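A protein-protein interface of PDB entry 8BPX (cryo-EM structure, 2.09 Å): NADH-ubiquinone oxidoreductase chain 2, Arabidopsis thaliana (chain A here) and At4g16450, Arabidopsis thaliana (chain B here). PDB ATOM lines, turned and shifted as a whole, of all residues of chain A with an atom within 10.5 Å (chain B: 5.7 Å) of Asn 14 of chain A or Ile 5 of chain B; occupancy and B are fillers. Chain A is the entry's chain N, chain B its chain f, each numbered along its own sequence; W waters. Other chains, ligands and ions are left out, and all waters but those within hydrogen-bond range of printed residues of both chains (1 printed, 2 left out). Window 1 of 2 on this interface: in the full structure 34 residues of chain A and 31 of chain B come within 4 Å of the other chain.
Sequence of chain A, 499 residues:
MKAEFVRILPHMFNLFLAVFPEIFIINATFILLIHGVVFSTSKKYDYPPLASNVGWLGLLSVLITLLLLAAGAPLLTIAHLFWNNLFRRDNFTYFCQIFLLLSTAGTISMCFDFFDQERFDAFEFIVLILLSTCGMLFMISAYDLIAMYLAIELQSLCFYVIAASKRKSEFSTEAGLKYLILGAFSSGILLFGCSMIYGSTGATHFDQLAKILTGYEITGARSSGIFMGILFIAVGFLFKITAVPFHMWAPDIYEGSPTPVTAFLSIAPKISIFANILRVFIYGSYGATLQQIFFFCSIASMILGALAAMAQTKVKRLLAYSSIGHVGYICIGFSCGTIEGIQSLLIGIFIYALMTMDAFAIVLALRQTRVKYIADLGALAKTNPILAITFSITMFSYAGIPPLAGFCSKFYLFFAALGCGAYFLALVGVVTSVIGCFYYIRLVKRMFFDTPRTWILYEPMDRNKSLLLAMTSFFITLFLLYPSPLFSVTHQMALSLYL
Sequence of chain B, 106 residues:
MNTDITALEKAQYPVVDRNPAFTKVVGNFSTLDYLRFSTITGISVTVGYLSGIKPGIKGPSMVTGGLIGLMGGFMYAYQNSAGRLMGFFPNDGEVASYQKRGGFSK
Water W1 lies within hydrogen-bond range of the backbone carbonyl oxygen (O) of Thr 6 of chain B, the backbone NH (N) of Leu 81 of chain A, the backbone carbonyl oxygen (O) of Asp 4 of chain B and the backbone NH (N) of His 80 of chain A.
ND1 of His 80 of chain A sits at hydrogen-bond distance from O of Thr 6 of chain B, 2.8 Å away. O of Pro 20 of chain B is in hydrogen-bond range of ND2 of Asn 14 of chain A (2.7 Å). The backbone carbonyl oxygen (O) of Ile 5 of chain B sits at hydrogen-bond distance from the backbone NH (N) of Ala 79 of chain A (3.0 Å). The side-chain amide oxygen (OD1) of Asn 14 of chain A is in hydrogen-bond range of the side-chain hydroxyl (OH) of Tyr 78 of chain B. N of Ala 79 of chain A sits at hydrogen-bond distance from O of Thr 6 of chain B, at 3.4 Å. ND2 of Asn 14 of chain A sits at hydrogen-bond distance from OD1 of Asn 19 of chain B (2.9 Å).
NH1 of Arg 18 of chain B lies within hydrogen-bond range of OG1 of Thr 6 of chain B (3.3 Å). NE1 of Trp 83 of chain A sits at hydrogen-bond distance from O of Leu 15 of chain A, 2.9 Å away.
Of the 23 printed residues of chain A, 8 touch a printed residue of chain B. Hydrophobic or aromatic side chains of chain A that line the printed part of chain B: Phe 13, Leu 15, Ile 78, Ala 79, His 80 and Leu 81. Printed residues of chain B that touch a printed residue of chain A: Thr 3, Asp 4, Ile 5, Thr 6, Ala 7, Asn 19, Pro 20, Tyr 78 and Met 86. Hydrophobic or aromatic side chains of chain B within 4 Å of the printed part of chain A: Ile 5, Ala 7, Pro 20, Tyr 78 and Met 86. Among the printed residues, no Asp or Glu carboxylate lies within 4 Å of a Lys or Arg side-chain nitrogen of the other chain.
Among the printed residues, merely in contact across the chains: Phe 13 of chain A with Tyr 78 of chain B (3.2 Å), Asn 14 of chain A with Ile 5 of chain B (3.8 Å), Asn 14 of chain A with Met 86 of chain B (3.4 Å), Leu 15 of chain A with Thr 3 of chain B (3.6 Å), Leu 15 of chain A with Asp 4 of chain B (3.9995 Å), Leu 15 of chain A with Ile 5 of chain B (3.7 Å), Thr 77 of chain A with Ala 7 of chain B (3.5 Å), Ile 78 of chain A with Ile 5 of chain B (3.4 Å), Ile 78 of chain A with Ala 7 of chain B (3.8 Å), Ile 78 of chain A with Met 86 of chain B (3.6 Å), Ala 79 of chain A with Asp 4 of chain B (3.2 Å), His 80 of chain A with Ala 7 of chain B (3.5 Å) and Leu 81 of chain A with Asp 4 of chain B (3.4 Å).
Of the printed residues of chain B, Asn 14 of chain A touches Ile 5 (3.8 Å), Asn 19 (2.9 Å), Pro 20 (2.7 Å), Tyr 78 (2.8 Å) and Met 86 (3.4 Å). Thr 6 of chain B touches just these residues of chain A: Ala 79 (3.4 Å) and His 80 (2.8 Å). Ala 7 of chain B touches three residues of chain A. Arg 18 of chain B touches none of the printed residues of chain A. Pro 20 of chain B touches just one residue of chain A: Asn 14. The nearest residue of chain B that does not touch Asn 14 of chain A is Ala 82 of chain B (4.5 Å). The nearest printed residue of chain B that does not touch Phe 13 of chain A is Asn 19 of chain B (5.9 Å).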
ATOM      1  N   MET A  12      -7.470  -7.295 -13.221  1.00  0.00           N
ATOM      2  CA  MET A  12      -8.467  -7.669 -12.221  1.00  0.00           C
ATOM      3  C   MET A  12      -8.206  -9.057 -11.636  1.00  0.00           C
ATOM      4  O   MET A  12      -8.226  -9.238 -10.419  1.00  0.00           O
ATOM      5  CB  MET A  12      -9.872  -7.617 -12.822  1.00  0.00           C
ATOM      6  CG  MET A  12     -10.937  -8.274 -11.957  1.00  0.00           C
ATOM      7  SD  MET A  12     -11.172  -7.450 -10.372  1.00  0.00           S
ATOM      8  CE  MET A  12     -12.281  -6.130 -10.847  1.00  0.00           C
ATOM      9  N   PHE A  13      -7.964 -10.035 -12.514  1.00  0.00           N
ATOM     10  CA  PHE A  13      -7.719 -11.400 -12.056  1.00  0.00           C
ATOM     11  C   PHE A  13      -6.516 -11.470 -11.124  1.00  0.00           C
ATOM     12  O   PHE A  13      -6.533 -12.210 -10.135  1.00  0.00           O
ATOM     13  CB  PHE A  13      -7.518 -12.332 -13.253  1.00  0.00           C
ATOM     14  CG  PHE A  13      -7.348 -13.778 -12.874  1.00  0.00           C
ATOM     15  CD1 PHE A  13      -6.090 -14.299 -12.602  1.00  0.00           C
ATOM     16  CD2 PHE A  13      -8.447 -14.615 -12.781  1.00  0.00           C
ATOM     17  CE1 PHE A  13      -5.935 -15.626 -12.244  1.00  0.00           C
ATOM     18  CE2 PHE A  13      -8.301 -15.943 -12.427  1.00  0.00           C
ATOM     19  CZ  PHE A  13      -7.041 -16.451 -12.157  1.00  0.00           C
ATOM     20  N   ASN A  14      -5.458 -10.713 -11.427  1.00  0.00           N
ATOM     21  CA  ASN A  14      -4.233 -10.806 -10.638  1.00  0.00           C
ATOM     22  C   ASN A  14      -4.431 -10.312  -9.212  1.00  0.00           C
ATOM     23  O   ASN A  14      -3.681 -10.712  -8.314  1.00  0.00           O
ATOM     24  CB  ASN A  14      -3.107 -10.029 -11.318  1.00  0.00           C
ATOM     25  CG  ASN A  14      -2.552 -10.754 -12.525  1.00  0.00           C
ATOM     26  OD1 ASN A  14      -2.685 -11.969 -12.643  1.00  0.00           O
ATOM     27  ND2 ASN A  14      -1.927 -10.010 -13.429  1.00  0.00           N
ATOM     28  N   LEU A  15      -5.419  -9.442  -8.982  1.00  0.00           N
ATOM     29  CA  LEU A  15      -5.730  -9.026  -7.617  1.00  0.00           C
ATOM     30  C   LEU A  15      -6.034 -10.221  -6.727  1.00  0.00           C
ATOM     31  O   LEU A  15      -5.688 -10.217  -5.542  1.00  0.00           O
ATOM     32  CB  LEU A  15      -6.915  -8.061  -7.604  1.00  0.00           C
ATOM     33  CG  LEU A  15      -6.917  -6.867  -8.556  1.00  0.00           C
ATOM     34  CD1 LEU A  15      -8.306  -6.259  -8.609  1.00  0.00           C
ATOM     35  CD2 LEU A  15      -5.892  -5.835  -8.129  1.00  0.00           C
ATOM     36  N   PHE A  16      -6.658 -11.259  -7.283  1.00  0.00           N
ATOM     37  CA  PHE A  16      -7.079 -12.412  -6.503  1.00  0.00           C
ATOM     38  C   PHE A  16      -5.938 -13.376  -6.201  1.00  0.00           C
ATOM     39  O   PHE A  16      -6.178 -14.412  -5.575  1.00  0.00           O
ATOM     40  CB  PHE A  16      -8.225 -13.134  -7.219  1.00  0.00           C
ATOM     41  CG  PHE A  16      -9.497 -12.330  -7.269  1.00  0.00           C
ATOM     42  CD1 PHE A  16      -9.686 -11.366  -8.246  1.00  0.00           C
ATOM     43  CD2 PHE A  16     -10.493 -12.518  -6.322  1.00  0.00           C
ATOM     44  CE1 PHE A  16     -10.848 -10.612  -8.286  1.00  0.00           C
ATOM     45  CE2 PHE A  16     -11.659 -11.767  -6.356  1.00  0.00           C
ATOM     46  CZ  PHE A  16     -11.836 -10.815  -7.338  1.00  0.00           C
ATOM     47  N   LEU A  17      -4.710 -13.057  -6.620  1.00  0.00           N
ATOM     48  CA  LEU A  17      -3.558 -13.837  -6.184  1.00  0.00           C
ATOM     49  C   LEU A  17      -3.395 -13.780  -4.671  1.00  0.00           C
ATOM     50  O   LEU A  17      -2.867 -14.720  -4.070  1.00  0.00           O
ATOM     51  CB  LEU A  17      -2.288 -13.337  -6.874  1.00  0.00           C
ATOM     52  CG  LEU A  17      -2.124 -13.743  -8.339  1.00  0.00           C
ATOM     53  CD1 LEU A  17      -0.956 -13.003  -8.977  1.00  0.00           C
ATOM     54  CD2 LEU A  17      -1.949 -15.249  -8.456  1.00  0.00           C
ATOM     55  N   ALA A  18      -3.860 -12.697  -4.041  1.00  0.00           N
ATOM     56  CA  ALA A  18      -3.811 -12.588  -2.587  1.00  0.00           C
ATOM     57  C   ALA A  18      -4.694 -13.616  -1.891  1.00  0.00           C
ATOM     58  O   ALA A  18      -4.526 -13.841  -0.688  1.00  0.00           O
ATOM     59  CB  ALA A  18      -4.225 -11.179  -2.153  1.00  0.00           C
ATOM     60  N   VAL A  19      -5.635 -14.236  -2.604  1.00  0.00           N
ATOM     61  CA  VAL A  19      -6.541 -15.198  -1.986  1.00  0.00           C
ATOM     62  C   VAL A  19      -6.563 -16.517  -2.749  1.00  0.00           C
ATOM     63  O   VAL A  19      -7.547 -17.259  -2.679  1.00  0.00           O
ATOM     64  CB  VAL A  19      -7.969 -14.627  -1.867  1.00  0.00           C
ATOM     65  CG1 VAL A  19      -8.049 -13.612  -0.741  1.00  0.00           C
ATOM     66  CG2 VAL A  19      -8.425 -14.025  -3.187  1.00  0.00           C
ATOM     67  N   PHE A  20      -5.489 -16.820  -3.485  1.00  0.00           N
ATOM     68  CA  PHE A  20      -5.418 -18.102  -4.189  1.00  0.00           C
ATOM     69  C   PHE A  20      -5.566 -19.312  -3.269  1.00  0.00           C
ATOM     70  O   PHE A  20      -6.358 -20.211  -3.602  1.00  0.00           O
ATOM     71  CB  PHE A  20      -4.118 -18.187  -5.002  1.00  0.00           C
ATOM     72  CG  PHE A  20      -4.301 -17.981  -6.482  1.00  0.00           C
ATOM     73  CD1 PHE A  20      -5.320 -17.185  -6.973  1.00  0.00           C
ATOM     74  CD2 PHE A  20      -3.456 -18.612  -7.386  1.00  0.00           C
ATOM     75  CE1 PHE A  20      -5.486 -17.008  -8.334  1.00  0.00           C
ATOM     76  CE2 PHE A  20      -3.619 -18.440  -8.750  1.00  0.00           C
ATOM     77  CZ  PHE A  20      -4.634 -17.636  -9.224  1.00  0.00           C
ATOM     78  N   PRO A  21      -4.832 -19.407  -2.129  1.00  0.00           N
ATOM     79  CA  PRO A  21      -4.951 -20.513  -1.186  1.00  0.00           C
ATOM     80  C   PRO A  21      -6.403 -20.744  -0.735  1.00  0.00           C
ATOM     81  O   PRO A  21      -6.866 -21.815  -0.866  1.00  0.00           O
ATOM     82  CB  PRO A  21      -4.108 -20.086   0.015  1.00  0.00           C
ATOM     83  CG  PRO A  21      -3.039 -19.225  -0.560  1.00  0.00           C
ATOM     84  CD  PRO A  21      -3.781 -18.471  -1.631  1.00  0.00           C
ATOM     85  N   ILE A  23      -9.271 -19.566  -2.129  1.00  0.00           N
ATOM     86  CA  ILE A  23     -10.108 -19.932  -3.271  1.00  0.00           C
ATOM     87  C   ILE A  23      -9.977 -21.420  -3.560  1.00  0.00           C
ATOM     88  O   ILE A  23     -10.978 -22.130  -3.736  1.00  0.00           O
ATOM     89  CB  ILE A  23      -9.733 -19.091  -4.505  1.00  0.00           C
ATOM     90  CG1 ILE A  23     -10.221 -17.650  -4.355  1.00  0.00           C
ATOM     91  CG2 ILE A  23     -10.304 -19.715  -5.776  1.00  0.00           C
ATOM     92  CD1 ILE A  23      -9.775 -16.751  -5.474  1.00  0.00           C
ATOM     93  N   GLY A  72       3.933 -19.023  -2.470  1.00  0.00           N
ATOM     94  CA  GLY A  72       3.567 -17.709  -2.959  1.00  0.00           C
ATOM     95  C   GLY A  72       3.621 -16.628  -1.899  1.00  0.00           C
ATOM     96  O   GLY A  72       2.719 -15.790  -1.820  1.00  0.00           O
ATOM     97  N   PRO A  74       5.412 -13.717  -1.277  1.00  0.00           N
ATOM     98  CA  PRO A  74       5.183 -12.315  -1.678  1.00  0.00           C
ATOM     99  C   PRO A  74       3.817 -12.069  -2.297  1.00  0.00           C
ATOM    100  O   PRO A  74       3.224 -11.008  -2.073  1.00  0.00           O
ATOM    101  CB  PRO A  74       6.309 -12.029  -2.682  1.00  0.00           C
ATOM    102  CG  PRO A  74       7.205 -13.199  -2.667  1.00  0.00           C
ATOM    103  CD  PRO A  74       6.494 -14.348  -2.053  1.00  0.00           C
ATOM    104  N   LEU A  75       3.295 -13.023  -3.068  1.00  0.00           N
ATOM    105  CA  LEU A  75       2.058 -12.780  -3.805  1.00  0.00           C
ATOM    106  C   LEU A  75       0.865 -12.591  -2.878  1.00  0.00           C
ATOM    107  O   LEU A  75      -0.109 -11.933  -3.257  1.00  0.00           O
ATOM    108  CB  LEU A  75       1.795 -13.920  -4.785  1.00  0.00           C
ATOM    109  CG  LEU A  75       2.885 -14.144  -5.834  1.00  0.00           C
ATOM    110  CD1 LEU A  75       2.561 -15.353  -6.682  1.00  0.00           C
ATOM    111  CD2 LEU A  75       3.061 -12.912  -6.699  1.00  0.00           C
ATOM    112  N   LEU A  76       0.919 -13.150  -1.667  1.00  0.00           N
ATOM    113  CA  LEU A  76      -0.173 -12.980  -0.719  1.00  0.00           C
ATOM    114  C   LEU A  76      -0.342 -11.527  -0.285  1.00  0.00           C
ATOM    115  O   LEU A  76      -1.405 -11.167   0.229  1.00  0.00           O
ATOM    116  CB  LEU A  76       0.051 -13.872   0.505  1.00  0.00           C
ATOM    117  CG  LEU A  76       0.187 -15.373   0.232  1.00  0.00           C
ATOM    118  CD1 LEU A  76       0.684 -16.103   1.470  1.00  0.00           C
ATOM    119  CD2 LEU A  76      -1.139 -15.951  -0.237  1.00  0.00           C
ATOM    120  N   THR A  77       0.677 -10.693  -0.477  1.00  0.00           N
ATOM    121  CA  THR A  77       0.609  -9.274  -0.153  1.00  0.00           C
ATOM    122  C   THR A  77       0.273  -8.405  -1.357  1.00  0.00           C
ATOM    123  O   THR A  77       0.278  -7.177  -1.239  1.00  0.00           O
ATOM    124  CB  THR A  77       1.933  -8.806   0.449  1.00  0.00           C
ATOM    125  OG1 THR A  77       2.992  -9.083  -0.469  1.00  0.00           O
ATOM    126  CG2 THR A  77       2.201  -9.528   1.759  1.00  0.00           C
ATOM    127  N   ILE A  78       0.005  -9.005  -2.516  1.00  0.00           N
ATOM    128  CA  ILE A  78      -0.331  -8.224  -3.697  1.00  0.00           C
ATOM    129  C   ILE A  78      -1.655  -7.500  -3.477  1.00  0.00           C
ATOM    130  O   ILE A  78      -2.539  -7.972  -2.748  1.00  0.00           O
ATOM    131  CB  ILE A  78      -0.379  -9.124  -4.946  1.00  0.00           C
ATOM    132  CG1 ILE A  78       0.192  -8.391  -6.159  1.00  0.00           C
ATOM    133  CG2 ILE A  78      -1.802  -9.588  -5.244  1.00  0.00           C
ATOM    134  CD1 ILE A  78       0.055  -9.168  -7.452  1.00  0.00           C
ATOM    135  N   ALA A  79      -1.778  -6.321  -4.093  1.00  0.00           N
ATOM    136  CA  ALA A  79      -3.011  -5.531  -4.074  1.00  0.00           C
ATOM    137  C   ALA A  79      -3.486  -5.252  -2.650  1.00  0.00           C
ATOM    138  O   ALA A  79      -4.683  -5.302  -2.357  1.00  0.00           O
ATOM    139  CB  ALA A  79      -4.112  -6.216  -4.888  1.00  0.00           C
ATOM    140  N   HIS A  80      -2.541  -4.946  -1.756  1.00  0.00           N
ATOM    141  CA  HIS A  80      -2.883  -4.809  -0.344  1.00  0.00           C
ATOM    142  C   HIS A  80      -3.816  -3.630  -0.089  1.00  0.00           C
ATOM    143  O   HIS A  80      -4.639  -3.687   0.828  1.00  0.00           O
ATOM    144  CB  HIS A  80      -1.616  -4.681   0.506  1.00  0.00           C
ATOM    145  CG  HIS A  80      -0.875  -3.394   0.314  1.00  0.00           C
ATOM    146  ND1 HIS A  80      -0.399  -2.984  -0.910  1.00  0.00           N
ATOM    147  CD2 HIS A  80      -0.530  -2.425   1.195  1.00  0.00           C
ATOM    148  CE1 HIS A  80       0.211  -1.821  -0.778  1.00  0.00           C
ATOM    149  NE2 HIS A  80       0.143  -1.458   0.490  1.00  0.00           N
ATOM    150  N   LEU A  81      -3.706  -2.558  -0.875  1.00  0.00           N
ATOM    151  CA  LEU A  81      -4.637  -1.444  -0.720  1.00  0.00           C
ATOM    152  C   LEU A  81      -6.054  -1.849  -1.107  1.00  0.00           C
ATOM    153  O   LEU A  81      -7.015  -1.482  -0.425  1.00  0.00           O
ATOM    154  CB  LEU A  81      -4.175  -0.248  -1.549  1.00  0.00           C
ATOM    155  CG  LEU A  81      -2.826   0.356  -1.162  1.00  0.00           C
ATOM    156  CD1 LEU A  81      -2.555   1.617  -1.971  1.00  0.00           C
ATOM    157  CD2 LEU A  81      -2.765   0.640   0.330  1.00  0.00           C
ATOM    158  N   PHE A  82      -6.199  -2.602  -2.200  1.00  0.00           N
ATOM    159  CA  PHE A  82      -7.519  -3.051  -2.629  1.00  0.00           C
ATOM    160  C   PHE A  82      -8.155  -3.970  -1.593  1.00  0.00           C
ATOM    161  O   PHE A  82      -9.363  -3.894  -1.343  1.00  0.00           O
ATOM    162  CB  PHE A  82      -7.411  -3.743  -3.990  1.00  0.00           C
ATOM    163  CG  PHE A  82      -8.679  -4.408  -4.449  1.00  0.00           C
ATOM    164  CD1 PHE A  82      -9.631  -3.693  -5.160  1.00  0.00           C
ATOM    165  CD2 PHE A  82      -8.907  -5.752  -4.196  1.00  0.00           C
ATOM    166  CE1 PHE A  82     -10.793  -4.301  -5.595  1.00  0.00           C
ATOM    167  CE2 PHE A  82     -10.069  -6.363  -4.624  1.00  0.00           C
ATOM    168  CZ  PHE A  82     -11.013  -5.637  -5.326  1.00  0.00           C
ATOM    169  N   TRP A  83      -7.359  -4.840  -0.977  1.00  0.00           N
ATOM    170  CA  TRP A  83      -7.851  -5.788   0.013  1.00  0.00           C
ATOM    171  C   TRP A  83      -7.833  -5.241   1.433  1.00  0.00           C
ATOM    172  O   TRP A  83      -8.207  -5.966   2.360  1.00  0.00           O
ATOM    173  CB  TRP A  83      -7.016  -7.073  -0.028  1.00  0.00           C
ATOM    174  CG  TRP A  83      -7.140  -7.850  -1.291  1.00  0.00           C
ATOM    175  CD1 TRP A  83      -6.177  -8.037  -2.234  1.00  0.00           C
ATOM    176  CD2 TRP A  83      -8.293  -8.566  -1.745  1.00  0.00           C
ATOM    177  NE1 TRP A  83      -6.659  -8.818  -3.253  1.00  0.00           N
ATOM    178  CE2 TRP A  83      -7.955  -9.160  -2.977  1.00  0.00           C
ATOM    179  CE3 TRP A  83      -9.577  -8.761  -1.232  1.00  0.00           C
ATOM    180  CZ2 TRP A  83      -8.855  -9.932  -3.705  1.00  0.00           C
ATOM    181  CZ3 TRP A  83     -10.471  -9.533  -1.955  1.00  0.00           C
ATOM    182  CH2 TRP A  83     -10.105 -10.108  -3.178  1.00  0.00           C
ATOM    183  N   PHE A  87      -8.985  -7.697   4.742  1.00  0.00           N
ATOM    184  CA  PHE A  87      -8.042  -8.500   5.516  1.00  0.00           C
ATOM    185  C   PHE A  87      -6.652  -7.890   5.349  1.00  0.00           C
ATOM    186  O   PHE A  87      -6.460  -6.926   4.604  1.00  0.00           O
ATOM    187  CB  PHE A  87      -8.074  -9.970   5.087  1.00  0.00           C
ATOM    188  CG  PHE A  87      -7.858 -10.181   3.619  1.00  0.00           C
ATOM    189  CD1 PHE A  87      -6.589 -10.094   3.065  1.00  0.00           C
ATOM    190  CD2 PHE A  87      -8.927 -10.473   2.788  1.00  0.00           C
ATOM    191  CE1 PHE A  87      -6.395 -10.289   1.714  1.00  0.00           C
ATOM    192  CE2 PHE A  87      -8.736 -10.674   1.436  1.00  0.00           C
ATOM    193  CZ  PHE A  87      -7.470 -10.578   0.898  1.00  0.00           C
ATOM    194  N   THR B   3      -9.170  -0.407  -8.724  1.00  0.00           N
ATOM    195  CA  THR B   3      -8.245  -1.488  -8.430  1.00  0.00           C
ATOM    196  C   THR B   3      -6.843  -0.920  -8.245  1.00  0.00           C
ATOM    197  O   THR B   3      -6.526   0.175  -8.714  1.00  0.00           O
ATOM    198  CB  THR B   3      -8.248  -2.549  -9.541  1.00  0.00           C
ATOM    199  OG1 THR B   3      -7.818  -1.956 -10.770  1.00  0.00           O
ATOM    200  CG2 THR B   3      -9.645  -3.117  -9.726  1.00  0.00           C
ATOM    201  N   ASP B   4      -6.010  -1.678  -7.534  1.00  0.00           N
ATOM    202  CA  ASP B   4      -4.623  -1.283  -7.289  1.00  0.00           C
ATOM    203  C   ASP B   4      -3.824  -2.547  -7.008  1.00  0.00           C
ATOM    204  O   ASP B   4      -3.948  -3.123  -5.924  1.00  0.00           O
ATOM    205  CB  ASP B   4      -4.530  -0.304  -6.125  1.00  0.00           C
ATOM    206  CG  ASP B   4      -3.208   0.441  -6.093  1.00  0.00           C
ATOM    207  OD1 ASP B   4      -2.282   0.046  -6.830  1.00  0.00           O
ATOM    208  OD2 ASP B   4      -3.092   1.418  -5.321  1.00  0.00           O
ATOM    209  N   ILE B   5      -2.998  -2.962  -7.970  1.00  0.00           N
ATOM    210  CA  ILE B   5      -2.210  -4.182  -7.825  1.00  0.00           C
ATOM    211  C   ILE B   5      -1.040  -4.024  -6.867  1.00  0.00           C
ATOM    212  O   ILE B   5      -0.459  -5.029  -6.446  1.00  0.00           O
ATOM    213  CB  ILE B   5      -1.701  -4.645  -9.206  1.00  0.00           C
ATOM    214  CG1 ILE B   5      -1.342  -6.137  -9.190  1.00  0.00           C
ATOM    215  CG2 ILE B   5      -0.495  -3.822  -9.635  1.00  0.00           C
ATOM    216  CD1 ILE B   5      -2.516  -7.051  -8.956  1.00  0.00           C
ATOM    217  N   THR B   6      -0.700  -2.791  -6.494  1.00  0.00           N
ATOM    218  CA  THR B   6       0.520  -2.496  -5.752  1.00  0.00           C
ATOM    219  C   THR B   6       0.639  -3.345  -4.494  1.00  0.00           C
ATOM    220  O   THR B   6      -0.254  -3.349  -3.643  1.00  0.00           O
ATOM    221  CB  THR B   6       0.548  -1.007  -5.393  1.00  0.00           C
ATOM    222  OG1 THR B   6       0.682  -0.235  -6.589  1.00  0.00           O
ATOM    223  CG2 THR B   6       1.708  -0.700  -4.463  1.00  0.00           C
ATOM    224  N   ALA B   7       1.750  -4.063  -4.382  1.00  0.00           N
ATOM    225  CA  ALA B   7       1.986  -4.970  -3.272  1.00  0.00           C
ATOM    226  C   ALA B   7       2.667  -4.245  -2.119  1.00  0.00           C
ATOM    227  O   ALA B   7       3.255  -3.175  -2.282  1.00  0.00           O
ATOM    228  CB  ALA B   7       2.836  -6.161  -3.715  1.00  0.00           C
ATOM    229  N   ARG B  18       3.733  -5.236 -15.055  1.00  0.00           N
ATOM    230  CA  ARG B  18       3.230  -4.969 -13.711  1.00  0.00           C
ATOM    231  C   ARG B  18       1.958  -5.757 -13.414  1.00  0.00           C
ATOM    232  O   ARG B  18       1.813  -6.325 -12.327  1.00  0.00           O
ATOM    233  CB  ARG B  18       2.983  -3.469 -13.545  1.00  0.00           C
ATOM    234  CG  ARG B  18       3.231  -2.942 -12.148  1.00  0.00           C
ATOM    235  CD  ARG B  18       3.035  -1.435 -12.090  1.00  0.00           C
ATOM    236  NE  ARG B  18       1.666  -1.067 -11.748  1.00  0.00           N
ATOM    237  CZ  ARG B  18       1.214  -0.906 -10.513  1.00  0.00           C
ATOM    238  NH1 ARG B  18       1.996  -1.079  -9.460  1.00  0.00           N
ATOM    239  NH2 ARG B  18      -0.058  -0.570 -10.328  1.00  0.00           N
ATOM    240  N   ASN B  19       1.024  -5.795 -14.361  1.00  0.00           N
ATOM    241  CA  ASN B  19      -0.262  -6.473 -14.186  1.00  0.00           C
ATOM    242  C   ASN B  19      -0.561  -7.287 -15.438  1.00  0.00           C
ATOM    243  O   ASN B  19      -1.396  -6.905 -16.264  1.00  0.00           O
ATOM    244  CB  ASN B  19      -1.374  -5.458 -13.902  1.00  0.00           C
ATOM    245  CG  ASN B  19      -2.614  -6.095 -13.300  1.00  0.00           C
ATOM    246  OD1 ASN B  19      -2.909  -7.266 -13.540  1.00  0.00           O
ATOM    247  ND2 ASN B  19      -3.348  -5.322 -12.512  1.00  0.00           N
ATOM    248  N   PRO B  20       0.119  -8.420 -15.614  1.00  0.00           N
ATOM    249  CA  PRO B  20      -0.030  -9.178 -16.862  1.00  0.00           C
ATOM    250  C   PRO B  20      -1.429  -9.750 -17.030  1.00  0.00           C
ATOM    251  O   PRO B  20      -2.047 -10.232 -16.080  1.00  0.00           O
ATOM    252  CB  PRO B  20       1.016 -10.290 -16.729  1.00  0.00           C
ATOM    253  CG  PRO B  20       1.250 -10.422 -15.266  1.00  0.00           C
ATOM    254  CD  PRO B  20       1.070  -9.056 -14.687  1.00  0.00           C
ATOM    255  N   ALA B  21      -1.913  -9.706 -18.268  1.00  0.00           N
ATOM    256  CA  ALA B  21      -3.215 -10.263 -18.598  1.00  0.00           C
ATOM    257  C   ALA B  21      -3.224 -11.775 -18.381  1.00  0.00           C
ATOM    258  O   ALA B  21      -2.184 -12.436 -18.379  1.00  0.00           O
ATOM    259  CB  ALA B  21      -3.580  -9.937 -20.044  1.00  0.00           C
ATOM    260  N   VAL B  25      -0.198 -14.438 -19.044  1.00  0.00           N
ATOM    261  CA  VAL B  25       0.386 -15.294 -18.014  1.00  0.00           C
ATOM    262  C   VAL B  25       0.361 -16.752 -18.458  1.00  0.00           C
ATOM    263  O   VAL B  25       1.347 -17.479 -18.295  1.00  0.00           O
ATOM    264  CB  VAL B  25      -0.336 -15.101 -16.666  1.00  0.00           C
ATOM    265  CG1 VAL B  25       0.209 -16.067 -15.627  1.00  0.00           C
ATOM    266  CG2 VAL B  25      -0.192 -13.669 -16.183  1.00  0.00           C
ATOM    267  N   TYR B  78       0.059 -20.814 -12.690  1.00  0.00           N
ATOM    268  CA  TYR B  78      -0.284 -19.413 -12.901  1.00  0.00           C
ATOM    269  C   TYR B  78       0.415 -18.526 -11.882  1.00  0.00           C
ATOM    270  O   TYR B  78       0.939 -17.462 -12.226  1.00  0.00           O
ATOM    271  CB  TYR B  78      -1.801 -19.223 -12.821  1.00  0.00           C
ATOM    272  CG  TYR B  78      -2.257 -17.840 -13.227  1.00  0.00           C
ATOM    273  CD1 TYR B  78      -2.125 -16.755 -12.364  1.00  0.00           C
ATOM    274  CD2 TYR B  78      -2.802 -17.614 -14.480  1.00  0.00           C
ATOM    275  CE1 TYR B  78      -2.527 -15.493 -12.742  1.00  0.00           C
ATOM    276  CE2 TYR B  78      -3.211 -16.356 -14.863  1.00  0.00           C
ATOM    277  CZ  TYR B  78      -3.070 -15.300 -13.993  1.00  0.00           C
ATOM    278  OH  TYR B  78      -3.478 -14.046 -14.372  1.00  0.00           O
ATOM    279  N   ALA B  82       2.920 -15.660 -13.260  1.00  0.00           N
ATOM    280  CA  ALA B  82       2.587 -14.272 -12.967  1.00  0.00           C
ATOM    281  C   ALA B  82       3.617 -13.639 -12.040  1.00  0.00           C
ATOM    282  O   ALA B  82       4.021 -12.492 -12.249  1.00  0.00           O
ATOM    283  CB  ALA B  82       1.185 -14.182 -12.364  1.00  0.00           C
ATOM    284  N   MET B  86       5.878 -10.374 -12.916  1.00  0.00           N
ATOM    285  CA  MET B  86       5.769  -9.214 -12.038  1.00  0.00           C
ATOM    286  C   MET B  86       7.059  -8.896 -11.294  1.00  0.00           C
ATOM    287  O   MET B  86       7.129  -7.857 -10.631  1.00  0.00           O
ATOM    288  CB  MET B  86       4.639  -9.433 -11.027  1.00  0.00           C
ATOM    289  CG  MET B  86       3.247  -9.529 -11.634  1.00  0.00           C
ATOM    290  SD  MET B  86       2.003  -9.815 -10.356  1.00  0.00           S
ATOM    291  CE  MET B  86       0.513  -9.256 -11.167  1.00  0.00           C
HETATM  292  O   HOH W   1      -2.552  -2.303  -3.326  1.00  0.00           O
